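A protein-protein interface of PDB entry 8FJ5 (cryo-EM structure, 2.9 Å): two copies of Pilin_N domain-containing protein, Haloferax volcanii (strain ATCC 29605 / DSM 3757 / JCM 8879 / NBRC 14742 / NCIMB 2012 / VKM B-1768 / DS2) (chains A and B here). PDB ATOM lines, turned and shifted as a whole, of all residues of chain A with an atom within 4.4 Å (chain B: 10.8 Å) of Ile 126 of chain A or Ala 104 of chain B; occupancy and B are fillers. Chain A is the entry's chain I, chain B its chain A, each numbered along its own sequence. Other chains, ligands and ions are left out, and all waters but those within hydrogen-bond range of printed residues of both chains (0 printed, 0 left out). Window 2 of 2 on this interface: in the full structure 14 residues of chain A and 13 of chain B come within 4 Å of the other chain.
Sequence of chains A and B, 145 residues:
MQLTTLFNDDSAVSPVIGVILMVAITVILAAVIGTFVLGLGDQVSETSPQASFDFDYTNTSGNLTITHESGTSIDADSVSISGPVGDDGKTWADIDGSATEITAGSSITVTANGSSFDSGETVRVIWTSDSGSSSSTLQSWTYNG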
ATOM      1  N   SER A  78       7.157   1.044  34.730  1.00  0.00           N
ATOM      2  CA  SER A  78       6.492   1.780  33.667  1.00  0.00           C
ATOM      3  C   SER A  78       5.126   2.315  34.067  1.00  0.00           C
ATOM      4  O   SER A  78       4.494   3.006  33.264  1.00  0.00           O
ATOM      5  CB  SER A  78       6.337   0.892  32.429  1.00  0.00           C
ATOM      6  OG  SER A  78       7.598   0.541  31.892  1.00  0.00           O
ATOM      7  N   VAL A  79       4.663   2.028  35.278  1.00  0.00           N
ATOM      8  CA  VAL A  79       3.313   2.362  35.716  1.00  0.00           C
ATOM      9  C   VAL A  79       3.425   3.240  36.952  1.00  0.00           C
ATOM     10  O   VAL A  79       4.139   2.900  37.901  1.00  0.00           O
ATOM     11  CB  VAL A  79       2.481   1.104  35.997  1.00  0.00           C
ATOM     12  CG1 VAL A  79       1.179   1.466  36.668  1.00  0.00           C
ATOM     13  CG2 VAL A  79       2.211   0.360  34.709  1.00  0.00           C
ATOM     14  N   SER A  80       2.724   4.371  36.945  1.00  0.00           N
ATOM     15  CA  SER A  80       2.679   5.292  38.070  1.00  0.00           C
ATOM     16  C   SER A  80       1.238   5.682  38.374  1.00  0.00           C
ATOM     17  O   SER A  80       0.353   5.562  37.523  1.00  0.00           O
ATOM     18  CB  SER A  80       3.511   6.546  37.794  1.00  0.00           C
ATOM     19  OG  SER A  80       2.924   7.337  36.778  1.00  0.00           O
ATOM     20  N   SER A  82      -1.361   8.678  39.581  1.00  0.00           N
ATOM     21  CA  SER A  82      -1.563  10.121  39.655  1.00  0.00           C
ATOM     22  C   SER A  82      -2.967  10.400  40.168  1.00  0.00           C
ATOM     23  O   SER A  82      -3.946   9.879  39.623  1.00  0.00           O
ATOM     24  CB  SER A  82      -1.358  10.784  38.294  1.00  0.00           C
ATOM     25  OG  SER A  82      -2.455  10.527  37.440  1.00  0.00           O
ATOM     26  N   ARG A 124      -5.822   7.917  38.440  1.00  0.00           N
ATOM     27  CA  ARG A 124      -5.459   7.296  37.175  1.00  0.00           C
ATOM     28  C   ARG A 124      -4.293   6.323  37.323  1.00  0.00           C
ATOM     29  O   ARG A 124      -3.467   6.429  38.230  1.00  0.00           O
ATOM     30  CB  ARG A 124      -5.103   8.358  36.134  1.00  0.00           C
ATOM     31  CG  ARG A 124      -6.277   9.171  35.654  1.00  0.00           C
ATOM     32  CD  ARG A 124      -5.851  10.216  34.649  1.00  0.00           C
ATOM     33  NE  ARG A 124      -6.996  10.943  34.114  1.00  0.00           N
ATOM     34  CZ  ARG A 124      -7.501  12.045  34.648  1.00  0.00           C
ATOM     35  NH1 ARG A 124      -6.983  12.584  35.739  1.00  0.00           N
ATOM     36  NH2 ARG A 124      -8.550  12.623  34.071  1.00  0.00           N
ATOM     37  N   VAL A 125      -4.247   5.363  36.402  1.00  0.00           N
ATOM     38  CA  VAL A 125      -3.111   4.465  36.216  1.00  0.00           C
ATOM     39  C   VAL A 125      -2.492   4.815  34.870  1.00  0.00           C
ATOM     40  O   VAL A 125      -3.190   4.837  33.850  1.00  0.00           O
ATOM     41  CB  VAL A 125      -3.534   2.988  36.269  1.00  0.00           C
ATOM     42  CG1 VAL A 125      -2.331   2.085  36.126  1.00  0.00           C
ATOM     43  CG2 VAL A 125      -4.275   2.689  37.557  1.00  0.00           C
ATOM     44  N   ILE A 126      -1.192   5.100  34.863  1.00  0.00           N
ATOM     45  CA  ILE A 126      -0.536   5.724  33.719  1.00  0.00           C
ATOM     46  C   ILE A 126       0.681   4.904  33.315  1.00  0.00           C
ATOM     47  O   ILE A 126       1.489   4.524  34.166  1.00  0.00           O
ATOM     48  CB  ILE A 126      -0.134   7.180  34.030  1.00  0.00           C
ATOM     49  CG1 ILE A 126      -1.377   8.014  34.324  1.00  0.00           C
ATOM     50  CG2 ILE A 126       0.650   7.788  32.879  1.00  0.00           C
ATOM     51  CD1 ILE A 126      -1.070   9.371  34.854  1.00  0.00           C
ATOM     52  N   TRP A 127       0.816   4.655  32.015  1.00  0.00           N
ATOM     53  CA  TRP A 127       1.957   3.943  31.451  1.00  0.00           C
ATOM     54  C   TRP A 127       2.866   4.929  30.723  1.00  0.00           C
ATOM     55  O   TRP A 127       2.383   5.804  30.000  1.00  0.00           O
ATOM     56  CB  TRP A 127       1.483   2.855  30.494  1.00  0.00           C
ATOM     57  CG  TRP A 127       2.587   2.174  29.760  1.00  0.00           C
ATOM     58  CD1 TRP A 127       3.377   1.168  30.220  1.00  0.00           C
ATOM     59  CD2 TRP A 127       3.034   2.460  28.431  1.00  0.00           C
ATOM     60  NE1 TRP A 127       4.284   0.801  29.257  1.00  0.00           N
ATOM     61  CE2 TRP A 127       4.095   1.584  28.150  1.00  0.00           C
ATOM     62  CE3 TRP A 127       2.639   3.375  27.451  1.00  0.00           C
ATOM     63  CZ2 TRP A 127       4.763   1.591  26.931  1.00  0.00           C
ATOM     64  CZ3 TRP A 127       3.305   3.383  26.246  1.00  0.00           C
ATOM     65  CH2 TRP A 127       4.354   2.498  25.995  1.00  0.00           C
ATOM     66  N   THR A 128       4.175   4.782  30.910  1.00  0.00           N
ATOM     67  CA  THR A 128       5.174   5.621  30.262  1.00  0.00           C
ATOM     68  C   THR A 128       6.197   4.741  29.556  1.00  0.00           C
ATOM     69  O   THR A 128       6.649   3.735  30.109  1.00  0.00           O
ATOM     70  CB  THR A 128       5.875   6.525  31.279  1.00  0.00           C
ATOM     71  OG1 THR A 128       4.899   7.299  31.983  1.00  0.00           O
ATOM     72  CG2 THR A 128       6.835   7.469  30.583  1.00  0.00           C
ATOM     73  N   SER A 135       3.074   8.375  26.509  1.00  0.00           N
ATOM     74  CA  SER A 135       2.352   8.018  27.719  1.00  0.00           C
ATOM     75  C   SER A 135       0.929   7.646  27.345  1.00  0.00           C
ATOM     76  O   SER A 135       0.437   7.995  26.271  1.00  0.00           O
ATOM     77  CB  SER A 135       2.352   9.160  28.741  1.00  0.00           C
ATOM     78  OG  SER A 135       3.653   9.417  29.232  1.00  0.00           O
ATOM     79  N   SER A 136       0.271   6.924  28.246  1.00  0.00           N
ATOM     80  CA  SER A 136      -1.123   6.568  28.055  1.00  0.00           C
ATOM     81  C   SER A 136      -1.768   6.362  29.414  1.00  0.00           C
ATOM     82  O   SER A 136      -1.093   6.075  30.404  1.00  0.00           O
ATOM     83  CB  SER A 136      -1.265   5.314  27.188  1.00  0.00           C
ATOM     84  OG  SER A 136      -2.624   5.008  26.947  1.00  0.00           O
ATOM     85  N   THR A 137      -3.084   6.521  29.453  1.00  0.00           N
ATOM     86  CA  THR A 137      -3.868   6.273  30.655  1.00  0.00           C
ATOM     87  C   THR A 137      -4.453   4.873  30.559  1.00  0.00           C
ATOM     88  O   THR A 137      -5.269   4.597  29.675  1.00  0.00           O
ATOM     89  CB  THR A 137      -4.974   7.313  30.824  1.00  0.00           C
ATOM     90  OG1 THR A 137      -4.392   8.613  30.963  1.00  0.00           O
ATOM     91  CG2 THR A 137      -5.807   7.012  32.050  1.00  0.00           C
ATOM     92  N   GLN B  50       1.108  14.311  17.712  1.00  0.00           N
ATOM     93  CA  GLN B  50      -0.192  13.652  17.730  1.00  0.00           C
ATOM     94  C   GLN B  50      -0.513  13.239  19.159  1.00  0.00           C
ATOM     95  O   GLN B  50       0.254  12.496  19.779  1.00  0.00           O
ATOM     96  CB  GLN B  50      -0.205  12.440  16.800  1.00  0.00           C
ATOM     97  CG  GLN B  50       0.076  12.775  15.345  1.00  0.00           C
ATOM     98  CD  GLN B  50      -0.004  11.566  14.436  1.00  0.00           C
ATOM     99  OE1 GLN B  50      -0.850  11.497  13.545  1.00  0.00           O
ATOM    100  NE2 GLN B  50       0.888  10.609  14.650  1.00  0.00           N
ATOM    101  N   ALA B  51      -1.645  13.713  19.671  1.00  0.00           N
ATOM    102  CA  ALA B  51      -2.052  13.436  21.041  1.00  0.00           C
ATOM    103  C   ALA B  51      -3.562  13.598  21.134  1.00  0.00           C
ATOM    104  O   ALA B  51      -4.205  14.142  20.235  1.00  0.00           O
ATOM    105  CB  ALA B  51      -1.337  14.353  22.033  1.00  0.00           C
ATOM    106  N   SER B  52      -4.121  13.118  22.241  1.00  0.00           N
ATOM    107  CA  SER B  52      -5.554  13.187  22.487  1.00  0.00           C
ATOM    108  C   SER B  52      -5.807  13.929  23.791  1.00  0.00           C
ATOM    109  O   SER B  52      -5.036  13.802  24.744  1.00  0.00           O
ATOM    110  CB  SER B  52      -6.169  11.787  22.543  1.00  0.00           C
ATOM    111  OG  SER B  52      -7.568  11.850  22.738  1.00  0.00           O
ATOM    112  N   PHE B  53      -6.882  14.712  23.820  1.00  0.00           N
ATOM    113  CA  PHE B  53      -7.230  15.532  24.972  1.00  0.00           C
ATOM    114  C   PHE B  53      -8.680  15.298  25.364  1.00  0.00           C
ATOM    115  O   PHE B  53      -9.518  14.944  24.533  1.00  0.00           O
ATOM    116  CB  PHE B  53      -7.010  17.027  24.696  1.00  0.00           C
ATOM    117  CG  PHE B  53      -5.578  17.393  24.461  1.00  0.00           C
ATOM    118  CD1 PHE B  53      -5.010  17.263  23.207  1.00  0.00           C
ATOM    119  CD2 PHE B  53      -4.793  17.860  25.498  1.00  0.00           C
ATOM    120  CE1 PHE B  53      -3.694  17.592  22.995  1.00  0.00           C
ATOM    121  CE2 PHE B  53      -3.480  18.194  25.289  1.00  0.00           C
ATOM    122  CZ  PHE B  53      -2.929  18.059  24.035  1.00  0.00           C
ATOM    123  N   ASP B  54      -8.966  15.512  26.644  1.00  0.00           N
ATOM    124  CA  ASP B  54     -10.300  15.343  27.204  1.00  0.00           C
ATOM    125  C   ASP B  54     -10.822  16.693  27.683  1.00  0.00           C
ATOM    126  O   ASP B  54     -10.166  17.366  28.484  1.00  0.00           O
ATOM    127  CB  ASP B  54     -10.270  14.335  28.352  1.00  0.00           C
ATOM    128  CG  ASP B  54     -11.646  14.024  28.897  1.00  0.00           C
ATOM    129  OD1 ASP B  54     -12.410  13.308  28.219  1.00  0.00           O
ATOM    130  OD2 ASP B  54     -11.957  14.479  30.016  1.00  0.00           O
ATOM    131  N   ILE B  66      -9.093  20.727  30.570  1.00  0.00           N
ATOM    132  CA  ILE B  66      -8.487  20.060  29.423  1.00  0.00           C
ATOM    133  C   ILE B  66      -7.349  19.189  29.934  1.00  0.00           C
ATOM    134  O   ILE B  66      -6.389  19.699  30.516  1.00  0.00           O
ATOM    135  CB  ILE B  66      -7.975  21.072  28.387  1.00  0.00           C
ATOM    136  CG1 ILE B  66      -9.049  22.115  28.089  1.00  0.00           C
ATOM    137  CG2 ILE B  66      -7.548  20.362  27.115  1.00  0.00           C
ATOM    138  CD1 ILE B  66      -8.519  23.350  27.426  1.00  0.00           C
ATOM    139  N   THR B  67      -7.440  17.882  29.692  1.00  0.00           N
ATOM    140  CA  THR B  67      -6.479  16.915  30.201  1.00  0.00           C
ATOM    141  C   THR B  67      -5.844  16.150  29.049  1.00  0.00           C
ATOM    142  O   THR B  67      -6.515  15.822  28.068  1.00  0.00           O
ATOM    143  CB  THR B  67      -7.144  15.925  31.171  1.00  0.00           C
ATOM    144  OG1 THR B  67      -7.915  16.646  32.138  1.00  0.00           O
ATOM    145  CG2 THR B  67      -6.104  15.098  31.898  1.00  0.00           C
ATOM    146  N   HIS B  68      -4.548  15.869  29.172  1.00  0.00           N
ATOM    147  CA  HIS B  68      -3.827  15.049  28.202  1.00  0.00           C
ATOM    148  C   HIS B  68      -4.128  13.582  28.481  1.00  0.00           C
ATOM    149  O   HIS B  68      -3.892  13.095  29.589  1.00  0.00           O
ATOM    150  CB  HIS B  68      -2.329  15.330  28.284  1.00  0.00           C
ATOM    151  CG  HIS B  68      -1.530  14.720  27.173  1.00  0.00           C
ATOM    152  ND1 HIS B  68      -0.944  13.477  27.271  1.00  0.00           N
ATOM    153  CD2 HIS B  68      -1.211  15.188  25.945  1.00  0.00           C
ATOM    154  CE1 HIS B  68      -0.302  13.205  26.151  1.00  0.00           C
ATOM    155  NE2 HIS B  68      -0.448  14.226  25.329  1.00  0.00           N
ATOM    156  N   GLU B  69      -4.647  12.874  27.478  1.00  0.00           N
ATOM    157  CA  GLU B  69      -5.032  11.475  27.622  1.00  0.00           C
ATOM    158  C   GLU B  69      -3.925  10.509  27.220  1.00  0.00           C
ATOM    159  O   GLU B  69      -3.476   9.710  28.043  1.00  0.00           O
ATOM    160  CB  GLU B  69      -6.282  11.181  26.785  1.00  0.00           C
ATOM    161  CG  GLU B  69      -7.593  11.318  27.518  1.00  0.00           C
ATOM    162  CD  GLU B  69      -8.778  11.210  26.580  1.00  0.00           C
ATOM    163  OE1 GLU B  69      -8.639  11.596  25.401  1.00  0.00           O
ATOM    164  OE2 GLU B  69      -9.846  10.732  27.016  1.00  0.00           O
ATOM    165  N   SER B  70      -3.483  10.561  25.966  1.00  0.00           N
ATOM    166  CA  SER B  70      -2.475   9.637  25.470  1.00  0.00           C
ATOM    167  C   SER B  70      -1.847  10.213  24.211  1.00  0.00           C
ATOM    168  O   SER B  70      -2.466  11.010  23.505  1.00  0.00           O
ATOM    169  CB  SER B  70      -3.072   8.254  25.188  1.00  0.00           C
ATOM    170  OG  SER B  70      -3.742   8.223  23.943  1.00  0.00           O
ATOM    171  N   GLY B  71      -0.615   9.792  23.937  1.00  0.00           N
ATOM    172  CA  GLY B  71       0.122  10.299  22.797  1.00  0.00           C
ATOM    173  C   GLY B  71       1.520  10.761  23.151  1.00  0.00           C
ATOM    174  O   GLY B  71       2.060  10.375  24.190  1.00  0.00           O
ATOM    175  N   THR B  72       2.110  11.600  22.306  1.00  0.00           N
ATOM    176  CA  THR B  72       3.479  12.048  22.506  1.00  0.00           C
ATOM    177  C   THR B  72       3.545  13.133  23.577  1.00  0.00           C
ATOM    178  O   THR B  72       2.535  13.710  23.983  1.00  0.00           O
ATOM    179  CB  THR B  72       4.075  12.571  21.199  1.00  0.00           C
ATOM    180  OG1 THR B  72       3.633  13.913  20.973  1.00  0.00           O
ATOM    181  CG2 THR B  72       3.648  11.704  20.031  1.00  0.00           C
ATOM    182  N   SER B  73       4.761  13.404  24.037  1.00  0.00           N
ATOM    183  CA  SER B  73       5.022  14.459  25.004  1.00  0.00           C
ATOM    184  C   SER B  73       5.259  15.769  24.272  1.00  0.00           C
ATOM    185  O   SER B  73       5.971  15.809  23.265  1.00  0.00           O
ATOM    186  CB  SER B  73       6.228  14.116  25.876  1.00  0.00           C
ATOM    187  OG  SER B  73       6.044  12.872  26.527  1.00  0.00           O
ATOM    188  N   ILE B  74       4.665  16.840  24.784  1.00  0.00           N
ATOM    189  CA  ILE B  74       4.657  18.125  24.102  1.00  0.00           C
ATOM    190  C   ILE B  74       5.218  19.193  25.028  1.00  0.00           C
ATOM    191  O   ILE B  74       4.900  19.239  26.220  1.00  0.00           O
ATOM    192  CB  ILE B  74       3.234  18.499  23.634  1.00  0.00           C
ATOM    193  CG1 ILE B  74       2.632  17.365  22.805  1.00  0.00           C
ATOM    194  CG2 ILE B  74       3.264  19.775  22.820  1.00  0.00           C
ATOM    195  CD1 ILE B  74       1.154  17.502  22.566  1.00  0.00           C
ATOM    196  N   TRP B  92       0.065  26.917  27.424  1.00  0.00           N
ATOM    197  CA  TRP B  92      -0.181  25.947  28.482  1.00  0.00           C
ATOM    198  C   TRP B  92       0.744  26.159  29.671  1.00  0.00           C
ATOM    199  O   TRP B  92       0.341  25.900  30.808  1.00  0.00           O
ATOM    200  CB  TRP B  92      -0.024  24.532  27.917  1.00  0.00           C
ATOM    201  CG  TRP B  92      -0.431  23.397  28.829  1.00  0.00           C
ATOM    202  CD1 TRP B  92       0.161  23.027  30.001  1.00  0.00           C
ATOM    203  CD2 TRP B  92      -1.499  22.467  28.612  1.00  0.00           C
ATOM    204  NE1 TRP B  92      -0.480  21.938  30.535  1.00  0.00           N
ATOM    205  CE2 TRP B  92      -1.500  21.572  29.699  1.00  0.00           C
ATOM    206  CE3 TRP B  92      -2.457  22.307  27.608  1.00  0.00           C
ATOM    207  CZ2 TRP B  92      -2.424  20.537  29.812  1.00  0.00           C
ATOM    208  CZ3 TRP B  92      -3.370  21.278  27.721  1.00  0.00           C
ATOM    209  CH2 TRP B  92      -3.347  20.407  28.813  1.00  0.00           C
ATOM    210  N   GLU B 101       6.452  20.058  30.492  1.00  0.00           N
ATOM    211  CA  GLU B 101       6.071  19.078  29.488  1.00  0.00           C
ATOM    212  C   GLU B 101       4.607  18.728  29.691  1.00  0.00           C
ATOM    213  O   GLU B 101       4.068  18.881  30.789  1.00  0.00           O
ATOM    214  CB  GLU B 101       6.925  17.804  29.578  1.00  0.00           C
ATOM    215  CG  GLU B 101       8.397  17.988  29.246  1.00  0.00           C
ATOM    216  CD  GLU B 101       8.642  18.342  27.792  1.00  0.00           C
ATOM    217  OE1 GLU B 101       7.862  17.891  26.928  1.00  0.00           O
ATOM    218  OE2 GLU B 101       9.614  19.077  27.512  1.00  0.00           O
ATOM    219  N   ILE B 102       3.964  18.266  28.627  1.00  0.00           N
ATOM    220  CA  ILE B 102       2.585  17.801  28.686  1.00  0.00           C
ATOM    221  C   ILE B 102       2.599  16.299  28.440  1.00  0.00           C
ATOM    222  O   ILE B 102       2.802  15.847  27.308  1.00  0.00           O
ATOM    223  CB  ILE B 102       1.684  18.525  27.677  1.00  0.00           C
ATOM    224  CG1 ILE B 102       1.972  20.024  27.673  1.00  0.00           C
ATOM    225  CG2 ILE B 102       0.223  18.283  28.001  1.00  0.00           C
ATOM    226  CD1 ILE B 102       1.312  20.758  26.542  1.00  0.00           C
ATOM    227  N   THR B 103       2.395  15.528  29.503  1.00  0.00           N
ATOM    228  CA  THR B 103       2.285  14.080  29.442  1.00  0.00           C
ATOM    229  C   THR B 103       0.909  13.680  29.956  1.00  0.00           C
ATOM    230  O   THR B 103       0.125  14.522  30.395  1.00  0.00           O
ATOM    231  CB  THR B 103       3.389  13.395  30.260  1.00  0.00           C
ATOM    232  OG1 THR B 103       3.162  13.616  31.655  1.00  0.00           O
ATOM    233  CG2 THR B 103       4.753  13.949  29.888  1.00  0.00           C
ATOM    234  N   ALA B 104       0.618  12.383  29.898  1.00  0.00           N
ATOM    235  CA  ALA B 104      -0.702  11.897  30.282  1.00  0.00           C
ATOM    236  C   ALA B 104      -0.995  12.223  31.741  1.00  0.00           C
ATOM    237  O   ALA B 104      -0.149  12.031  32.619  1.00  0.00           O
ATOM    238  CB  ALA B 104      -0.805  10.393  30.043  1.00  0.00           C
ATOM    239  N   GLY B 105      -2.202  12.717  31.997  1.00  0.00           N
ATOM    240  CA  GLY B 105      -2.594  13.138  33.322  1.00  0.00           C
ATOM    241  C   GLY B 105      -2.418  14.610  33.612  1.00  0.00           C
ATOM    242  O   GLY B 105      -2.768  15.050  34.711  1.00  0.00           O
ATOM    243  N   SER B 106      -1.888  15.382  32.667  1.00  0.00           N
ATOM    244  CA  SER B 106      -1.683  16.811  32.851  1.00  0.00           C
ATOM    245  C   SER B 106      -2.927  17.572  32.423  1.00  0.00           C
ATOM    246  O   SER B 106      -3.505  17.293  31.372  1.00  0.00           O
ATOM    247  CB  SER B 106      -0.476  17.288  32.044  1.00  0.00           C
ATOM    248  OG  SER B 106       0.718  16.678  32.491  1.00  0.00           O
ATOM    249  N   SER B 107      -3.338  18.542  33.237  1.00  0.00           N
ATOM    250  CA  SER B 107      -4.571  19.260  32.955  1.00  0.00           C
ATOM    251  C   SER B 107      -4.434  20.730  33.320  1.00  0.00           C
ATOM    252  O   SER B 107      -3.630  21.113  34.171  1.00  0.00           O
ATOM    253  CB  SER B 107      -5.761  18.641  33.697  1.00  0.00           C
ATOM    254  OG  SER B 107      -5.485  18.482  35.074  1.00  0.00           O
ATOM    255  N   ILE B 108      -5.246  21.549  32.651  1.00  0.00           N
ATOM    256  CA  ILE B 108      -5.407  22.964  32.950  1.00  0.00           C
ATOM    257  C   ILE B 108      -6.899  23.259  33.034  1.00  0.00           C
ATOM    258  O   ILE B 108      -7.734  22.494  32.552  1.00  0.00           O
ATOM    259  CB  ILE B 108      -4.736  23.875  31.902  1.00  0.00           C
ATOM    260  CG1 ILE B 108      -5.277  23.560  30.508  1.00  0.00           C
ATOM    261  CG2 ILE B 108      -3.228  23.729  31.948  1.00  0.00           C
ATOM    262  CD1 ILE B 108      -4.896  24.575  29.469  1.00  0.00           C
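Of the 23 printed residues of chain B, 4 touch a printed residue of chain A.
Hydrophobic or aromatic side chains of chain A that line the printed part of chain B: Ile 126.
Along chain A the printed residues that touch a printed residue of chain B span positions 126 to 137.
Among the printed residues, 7 pairs touch across the chains.
OE1 of Glu 69 of chain B sits at hydrogen-bond distance from OG of Ser 52 of chain B, at 2.9 Å.
The backbone NH (N) of Ser 52 of chain B sits at hydrogen-bond distance from the backbone carbonyl oxygen (O) of Ser 70 of chain B (3.0 Å).
The backbone NH (N) of Ala 104 of chain B sits at hydrogen-bond distance from a ring nitrogen (ND1) of His 68 of chain B, at 3.2 Å.
The backbone carbonyl oxygen of Ile 126 of chain A is in hydrogen-bond range of the backbone NH of Ser 80 of chain A (3.0 Å).
The backbone NH (N) of Trp 127 of chain A is in hydrogen-bond range of the backbone carbonyl oxygen (O) of Ser 136 of chain A (2.9 Å).
Among the printed residues, pairs that only touch across the chains: Ile 126 of chain A with Ala 104 of chain B (3.6 Å), Ser 135 of chain A with Ser 70 of chain B (3.4 Å), Ser 135 of chain A with Ala 104 of chain B (3.6 Å), Ser 136 of chain A with Glu 69 of chain B (3.9 Å) and Ser 136 of chain A with Ser 70 of chain B (3.7 Å).
Ala 104 of chain B touches two residues of chain A.
No residue of chain B comes within 4 Å of Ser 80 of chain A.
No residue of chain B comes within 4 Å of Val 125 of chain A.
Ser 135 of chain A touches just these residues of chain B: Ser 70 (3.4 Å), Gly 71 (3.1 Å) and Ala 104 (3.6 Å).
Ser 136 of chain A touches just these residues of chain B: Glu 69 (3.9 Å) and Ser 70 (3.7 Å).
Of the printed residues of chain A, Ser 70 of chain B touches Ser 135 (3.4 Å) and Ser 136 (3.7 Å).
Printed residues of chain A within 4 Å of Gly 71 of chain B: Ser 135.
Of the printed residues of chain A, Glu 69 of chain B touches Ser 136 (3.9 Å) and Thr 137 (3.3 Å).
O of Glu 69 of chain B is in hydrogen-bond range of OG1 of Thr 137 of chain A (3.3 Å).
O of Ser 135 of chain A is in hydrogen-bond range of N of Gly 71 of chain B, 3.1 Å away.
No position is printed for both chains.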
